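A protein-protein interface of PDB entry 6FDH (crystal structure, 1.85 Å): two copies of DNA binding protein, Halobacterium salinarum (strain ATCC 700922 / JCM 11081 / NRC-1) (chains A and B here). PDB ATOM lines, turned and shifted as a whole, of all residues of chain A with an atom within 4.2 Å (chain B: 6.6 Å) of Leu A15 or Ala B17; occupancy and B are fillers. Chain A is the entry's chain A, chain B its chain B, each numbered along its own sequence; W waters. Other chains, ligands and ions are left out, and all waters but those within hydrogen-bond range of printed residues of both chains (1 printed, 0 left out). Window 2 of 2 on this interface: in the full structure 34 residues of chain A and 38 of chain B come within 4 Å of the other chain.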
ATOM      1  N   ALA A  12      27.322   1.407  11.160  1.00  0.00           N
ATOM      2  CA  ALA A  12      27.059  -0.009  10.950  1.00  0.00           C
ATOM      3  C   ALA A  12      25.584  -0.342  10.785  1.00  0.00           C
ATOM      4  O   ALA A  12      25.255  -1.472  10.420  1.00  0.00           O
ATOM      5  CB  ALA A  12      27.617  -0.829  12.118  1.00  0.00           C
ATOM      6  N   ARG A  13      24.679   0.601  11.047  1.00  0.00           N
ATOM      7  CA  ARG A  13      23.265   0.278  10.916  1.00  0.00           C
ATOM      8  C   ARG A  13      22.823   0.141   9.461  1.00  0.00           C
ATOM      9  O   ARG A  13      21.705  -0.326   9.226  1.00  0.00           O
ATOM     10  CB  ARG A  13      22.424   1.333  11.652  1.00  0.00           C
ATOM     11  CG  ARG A  13      22.551   1.218  13.179  1.00  0.00           C
ATOM     12  CD  ARG A  13      21.663   2.198  13.962  1.00  0.00           C
ATOM     13  NE  ARG A  13      21.663   1.877  15.392  1.00  0.00           N
ATOM     14  CZ  ARG A  13      20.856   2.419  16.302  1.00  0.00           C
ATOM     15  NH1 ARG A  13      19.965   3.337  15.951  1.00  0.00           N
ATOM     16  NH2 ARG A  13      20.946   2.050  17.578  1.00  0.00           N
ATOM     17  N   ASP A  14      23.674   0.474   8.492  1.00  0.00           N
ATOM     18  CA  ASP A  14      23.331   0.374   7.076  1.00  0.00           C
ATOM     19  C   ASP A  14      23.783  -0.930   6.432  1.00  0.00           C
ATOM     20  O   ASP A  14      23.620  -1.094   5.221  1.00  0.00           O
ATOM     21  CB  ASP A  14      23.951   1.535   6.301  1.00  0.00           C
ATOM     22  CG  ASP A  14      23.285   2.850   6.607  1.00  0.00           C
ATOM     23  OD1 ASP A  14      22.077   2.829   6.928  1.00  0.00           O
ATOM     24  OD2 ASP A  14      23.961   3.900   6.522  1.00  0.00           O
ATOM     25  N   LEU A  15      24.375  -1.836   7.194  1.00  0.00           N
ATOM     26  CA  LEU A  15      24.865  -3.083   6.622  1.00  0.00           C
ATOM     27  C   LEU A  15      23.724  -3.939   6.076  1.00  0.00           C
ATOM     28  O   LEU A  15      22.576  -3.858   6.527  1.00  0.00           O
ATOM     29  CB  LEU A  15      25.634  -3.881   7.672  1.00  0.00           C
ATOM     30  CG  LEU A  15      26.900  -3.244   8.235  1.00  0.00           C
ATOM     31  CD1 LEU A  15      27.464  -4.084   9.365  1.00  0.00           C
ATOM     32  CD2 LEU A  15      27.949  -3.035   7.163  1.00  0.00           C
ATOM     33  N   THR A  16      24.050  -4.778   5.102  1.00  0.00           N
ATOM     34  CA  THR A  16      23.089  -5.746   4.600  1.00  0.00           C
ATOM     35  C   THR A  16      22.846  -6.844   5.637  1.00  0.00           C
ATOM     36  O   THR A  16      23.657  -7.071   6.541  1.00  0.00           O
ATOM     37  CB  THR A  16      23.585  -6.400   3.316  1.00  0.00           C
ATOM     38  OG1 THR A  16      24.727  -7.197   3.629  1.00  0.00           O
ATOM     39  CG2 THR A  16      23.984  -5.359   2.278  1.00  0.00           C
ATOM     40  N   ALA A  17      21.705  -7.526   5.494  1.00  0.00           N
ATOM     41  CA  ALA A  17      21.375  -8.628   6.392  1.00  0.00           C
ATOM     42  C   ALA A  17      22.480  -9.675   6.394  1.00  0.00           C
ATOM     43  O   ALA A  17      22.874 -10.178   7.452  1.00  0.00           O
ATOM     44  CB  ALA A  17      20.030  -9.242   5.979  1.00  0.00           C
ATOM     45  N   GLN A  19      25.686  -9.235   5.743  1.00  0.00           N
ATOM     46  CA  GLN A  19      26.830  -8.716   6.484  1.00  0.00           C
ATOM     47  C   GLN A  19      26.580  -8.745   7.992  1.00  0.00           C
ATOM     48  O   GLN A  19      27.464  -9.119   8.768  1.00  0.00           O
ATOM     49  CB  GLN A  19      27.166  -7.303   6.018  1.00  0.00           C
ATOM     50  CG  GLN A  19      27.825  -7.278   4.648  1.00  0.00           C
ATOM     51  CD  GLN A  19      27.905  -5.902   4.056  1.00  0.00           C
ATOM     52  OE1 GLN A  19      27.155  -4.990   4.441  1.00  0.00           O
ATOM     53  NE2 GLN A  19      28.795  -5.744   3.079  1.00  0.00           N
ATOM     54  N   LYS A  20      25.383  -8.344   8.433  1.00  0.00           N
ATOM     55  CA  LYS A  20      25.097  -8.407   9.861  1.00  0.00           C
ATOM     56  C   LYS A  20      25.173  -9.834  10.381  1.00  0.00           C
ATOM     57  O   LYS A  20      25.560 -10.055  11.535  1.00  0.00           O
ATOM     58  CB  LYS A  20      23.726  -7.828  10.147  1.00  0.00           C
ATOM     59  CG  LYS A  20      23.632  -6.370   9.815  1.00  0.00           C
ATOM     60  CD  LYS A  20      22.256  -5.841  10.190  1.00  0.00           C
ATOM     61  CE  LYS A  20      22.084  -4.430   9.691  1.00  0.00           C
ATOM     62  NZ  LYS A  20      22.647  -3.409  10.639  1.00  0.00           N
ATOM     63  N   LEU A  23      28.652 -10.791  11.172  1.00  0.00           N
ATOM     64  CA  LEU A  23      29.069 -10.214  12.443  1.00  0.00           C
ATOM     65  C   LEU A  23      28.486 -11.011  13.600  1.00  0.00           C
ATOM     66  O   LEU A  23      29.168 -11.250  14.601  1.00  0.00           O
ATOM     67  CB  LEU A  23      28.654  -8.742  12.530  1.00  0.00           C
ATOM     68  CG  LEU A  23      29.209  -7.747  11.496  1.00  0.00           C
ATOM     69  CD1 LEU A  23      28.744  -6.334  11.814  1.00  0.00           C
ATOM     70  CD2 LEU A  23      30.727  -7.796  11.420  1.00  0.00           C
ATOM     71  N   LYS A  63      35.703  -1.938   6.237  1.00  0.00           N
ATOM     72  CA  LYS A  63      34.921  -1.058   7.091  1.00  0.00           C
ATOM     73  C   LYS A  63      35.452  -0.980   8.517  1.00  0.00           C
ATOM     74  O   LYS A  63      34.964  -0.154   9.298  1.00  0.00           O
ATOM     75  CB  LYS A  63      33.471  -1.533   7.092  1.00  0.00           C
ATOM     76  CG  LYS A  63      32.755  -1.319   5.764  1.00  0.00           C
ATOM     77  CD  LYS A  63      31.433  -2.073   5.747  1.00  0.00           C
ATOM     78  CE  LYS A  63      30.764  -2.026   4.389  1.00  0.00           C
ATOM     79  NZ  LYS A  63      30.358  -0.632   4.039  1.00  0.00           N
ATOM     80  N   LEU A  65      35.272  -3.460  10.763  1.00  0.00           N
ATOM     81  CA  LEU A  65      34.426  -4.229  11.661  1.00  0.00           C
ATOM     82  C   LEU A  65      34.956  -5.623  11.936  1.00  0.00           C
ATOM     83  O   LEU A  65      34.580  -6.225  12.950  1.00  0.00           O
ATOM     84  CB  LEU A  65      33.006  -4.327  11.090  1.00  0.00           C
ATOM     85  CG  LEU A  65      32.421  -2.951  10.779  1.00  0.00           C
ATOM     86  CD1 LEU A  65      31.094  -3.078  10.077  1.00  0.00           C
ATOM     87  CD2 LEU A  65      32.259  -2.122  12.042  1.00  0.00           C
ATOM     88  N   LEU B  15      14.897 -12.191   4.295  1.00  0.00           N
ATOM     89  CA  LEU B  15      14.469 -10.797   4.218  1.00  0.00           C
ATOM     90  C   LEU B  15      15.657  -9.841   4.239  1.00  0.00           C
ATOM     91  O   LEU B  15      16.720 -10.142   4.795  1.00  0.00           O
ATOM     92  CB  LEU B  15      13.543 -10.481   5.392  1.00  0.00           C
ATOM     93  CG  LEU B  15      12.241 -11.261   5.529  1.00  0.00           C
ATOM     94  CD1 LEU B  15      11.606 -10.942   6.877  1.00  0.00           C
ATOM     95  CD2 LEU B  15      11.299 -10.931   4.375  1.00  0.00           C
ATOM     96  N   THR B  16      15.468  -8.667   3.640  1.00  0.00           N
ATOM     97  CA  THR B  16      16.474  -7.613   3.717  1.00  0.00           C
ATOM     98  C   THR B  16      16.535  -7.055   5.132  1.00  0.00           C
ATOM     99  O   THR B  16      15.607  -7.213   5.921  1.00  0.00           O
ATOM    100  CB  THR B  16      16.163  -6.467   2.757  1.00  0.00           C
ATOM    101  OG1 THR B  16      14.968  -5.808   3.183  1.00  0.00           O
ATOM    102  CG2 THR B  16      15.995  -6.976   1.350  1.00  0.00           C
ATOM    103  N   ALA B  17      17.660  -6.406   5.448  1.00  0.00           N
ATOM    104  CA  ALA B  17      17.800  -5.742   6.743  1.00  0.00           C
ATOM    105  C   ALA B  17      16.674  -4.742   6.965  1.00  0.00           C
ATOM    106  O   ALA B  17      16.125  -4.637   8.069  1.00  0.00           O
ATOM    107  CB  ALA B  17      19.155  -5.034   6.817  1.00  0.00           C
ATOM    108  N   PHE B  18      16.320  -3.995   5.920  1.00  0.00           N
ATOM    109  CA  PHE B  18      15.254  -3.001   6.027  1.00  0.00           C
ATOM    110  C   PHE B  18      13.924  -3.657   6.364  1.00  0.00           C
ATOM    111  O   PHE B  18      13.197  -3.212   7.263  1.00  0.00           O
ATOM    112  CB  PHE B  18      15.179  -2.233   4.704  1.00  0.00           C
ATOM    113  CG  PHE B  18      14.243  -1.047   4.717  1.00  0.00           C
ATOM    114  CD1 PHE B  18      14.624   0.151   5.305  1.00  0.00           C
ATOM    115  CD2 PHE B  18      13.007  -1.116   4.098  1.00  0.00           C
ATOM    116  CE1 PHE B  18      13.774   1.241   5.300  1.00  0.00           C
ATOM    117  CE2 PHE B  18      12.151  -0.020   4.085  1.00  0.00           C
ATOM    118  CZ  PHE B  18      12.545   1.161   4.691  1.00  0.00           C
ATOM    119  N   GLN B  19      13.582  -4.722   5.650  1.00  0.00           N
ATOM    120  CA  GLN B  19      12.355  -5.451   5.950  1.00  0.00           C
ATOM    121  C   GLN B  19      12.368  -6.043   7.355  1.00  0.00           C
ATOM    122  O   GLN B  19      11.346  -6.033   8.042  1.00  0.00           O
ATOM    123  CB  GLN B  19      12.155  -6.549   4.908  1.00  0.00           C
ATOM    124  CG  GLN B  19      11.720  -6.027   3.564  1.00  0.00           C
ATOM    125  CD  GLN B  19      11.874  -7.053   2.476  1.00  0.00           C
ATOM    126  OE1 GLN B  19      12.517  -8.104   2.670  1.00  0.00           O
ATOM    127  NE2 GLN B  19      11.298  -6.761   1.311  1.00  0.00           N
ATOM    128  N   LYS B  20      13.503  -6.622   7.788  1.00  0.00           N
ATOM    129  CA  LYS B  20      13.566  -7.146   9.152  1.00  0.00           C
ATOM    130  C   LYS B  20      13.343  -6.034  10.171  1.00  0.00           C
ATOM    131  O   LYS B  20      12.679  -6.243  11.194  1.00  0.00           O
ATOM    132  CB  LYS B  20      14.908  -7.827   9.423  1.00  0.00           C
ATOM    133  CG  LYS B  20      15.087  -9.146   8.724  1.00  0.00           C
ATOM    134  CD  LYS B  20      16.393  -9.795   9.136  1.00  0.00           C
ATOM    135  CE  LYS B  20      16.881 -10.710   8.048  1.00  0.00           C
ATOM    136  NZ  LYS B  20      16.084 -11.975   7.944  1.00  0.00           N
ATOM    137  N   ASN B  21      13.895  -4.848   9.904  1.00  0.00           N
ATOM    138  CA  ASN B  21      13.739  -3.720  10.823  1.00  0.00           C
ATOM    139  C   ASN B  21      12.285  -3.265  10.905  1.00  0.00           C
ATOM    140  O   ASN B  21      11.816  -2.857  11.976  1.00  0.00           O
ATOM    141  CB  ASN B  21      14.655  -2.570  10.397  1.00  0.00           C
ATOM    142  CG  ASN B  21      16.139  -2.875  10.627  1.00  0.00           C
ATOM    143  OD1 ASN B  21      16.490  -3.723  11.440  1.00  0.00           O
ATOM    144  ND2 ASN B  21      17.012  -2.169   9.911  1.00  0.00           N
ATOM    145  N   ILE B  22      11.557  -3.317   9.789  1.00  0.00           N
ATOM    146  CA  ILE B  22      10.123  -3.056   9.827  1.00  0.00           C
ATOM    147  C   ILE B  22       9.437  -4.046  10.761  1.00  0.00           C
ATOM    148  O   ILE B  22       8.640  -3.665  11.625  1.00  0.00           O
ATOM    149  CB  ILE B  22       9.522  -3.121   8.415  1.00  0.00           C
ATOM    150  CG1 ILE B  22      10.013  -1.985   7.542  1.00  0.00           C
ATOM    151  CG2 ILE B  22       7.991  -3.103   8.465  1.00  0.00           C
ATOM    152  CD1 ILE B  22       9.590  -2.153   6.091  1.00  0.00           C
ATOM    153  N   TYR B  44      17.978   4.572  11.777  1.00  0.00           N
ATOM    154  CA  TYR B  44      19.040   4.810  10.804  1.00  0.00           C
ATOM    155  C   TYR B  44      19.744   6.139  11.013  1.00  0.00           C
ATOM    156  O   TYR B  44      20.874   6.308  10.540  1.00  0.00           O
ATOM    157  CB  TYR B  44      18.495   4.773   9.378  1.00  0.00           C
ATOM    158  CG  TYR B  44      18.086   3.406   8.913  1.00  0.00           C
ATOM    159  CD1 TYR B  44      19.044   2.424   8.704  1.00  0.00           C
ATOM    160  CD2 TYR B  44      16.760   3.089   8.681  1.00  0.00           C
ATOM    161  CE1 TYR B  44      18.696   1.153   8.278  1.00  0.00           C
ATOM    162  CE2 TYR B  44      16.395   1.815   8.259  1.00  0.00           C
ATOM    163  CZ  TYR B  44      17.370   0.856   8.062  1.00  0.00           C
ATOM    164  OH  TYR B  44      17.018  -0.411   7.652  1.00  0.00           O
ATOM    165  N   ARG B  52      10.726   3.983  -0.591  1.00  0.00           N
ATOM    166  CA  ARG B  52      11.360   2.786  -0.062  1.00  0.00           C
ATOM    167  C   ARG B  52      10.477   2.071   0.943  1.00  0.00           C
ATOM    168  O   ARG B  52      10.342   0.845   0.886  1.00  0.00           O
ATOM    169  CB  ARG B  52      12.698   3.137   0.593  1.00  0.00           C
ATOM    170  CG  ARG B  52      13.559   1.927   0.874  1.00  0.00           C
ATOM    171  CD  ARG B  52      14.846   2.245   1.647  1.00  0.00           C
ATOM    172  NE  ARG B  52      15.684   1.047   1.784  1.00  0.00           N
ATOM    173  CZ  ARG B  52      16.692   0.924   2.643  1.00  0.00           C
ATOM    174  NH1 ARG B  52      17.004   1.927   3.461  1.00  0.00           N
ATOM    175  NH2 ARG B  52      17.390  -0.209   2.681  1.00  0.00           N
HETATM  176  O   HOH W   1      19.976  -2.799  10.464  1.00  0.00           O
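Printed residues of chain A that touch a printed residue of chain B: Arg A13, Asp A14, Leu A15 and Ala A17. Hydrophobic or aromatic side chains of chain A that line the printed part of chain B: Ala A17. Of the 10 printed residues of chain B, 3 touch a printed residue of chain A. Printed residues of chain B that touch a printed residue of chain A: Leu B15, Ala B17 and Tyr B44. Hydrophobic or aromatic side chains of chain B that line the printed part of chain A: Ala B17 and Tyr B44. Along chain B the printed residues that touch a printed residue of chain A span positions 15 to 44. Among the printed residues, 5 pairs touch across the chains.
Water W1 lies within hydrogen-bond range of NZ of Lys A20 (2.7 Å), ND2 of Asn B21 (3.1 Å) and O of Arg A13 (3.3 Å).
The side-chain amide nitrogen of Asn B21 lies within hydrogen-bond range of the side-chain hydroxyl of Tyr B44 (2.9 Å). ND2 of Asn B21 lies close to O of Ala B17, 3.2 Å away.
Leu A15 touches Ala B17, and with the chains exchanged Ala A17 touches Leu B15. Ala A17 touches its own counterpart, Ala B17. 5 positions are printed for both chains. Of the 5 pairs that touch across the chains among the printed residues, 3 have their exchanged pair printed and touching as well.
Of chain B, only Ala B17 comes within 4 Å of Leu A15. Of chain A, only Leu A15 and Ala A17 come within 4 Å of Ala B17. Of the printed residues of chain A, Tyr B44 touches Arg A13 and Asp A14. Of the printed residues of chain A, Leu B15 touches Ala A17. Printed residues of chain B within 4 Å of Asp A14: Tyr B44. The nearest residue of chain B that does not touch Leu A15 is Phe B18 (6.3 Å). The nearest residue of chain A that does not touch Ala B17 is Lys A20 (4.1 Å). The nearest printed residue of chain A that does not touch Tyr B44 is Lys A20 (6.5 Å).
Among the printed residues, merely in contact across the chains: Arg A13 with Tyr B44 (3.5 Å), Asp A14 with Tyr B44 (3.5 Å), Leu A15 with Ala B17 (3.6 Å), Ala A17 with Leu B15 (3.6 Å) and Ala A17 with Ala B17 (3.7 Å).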
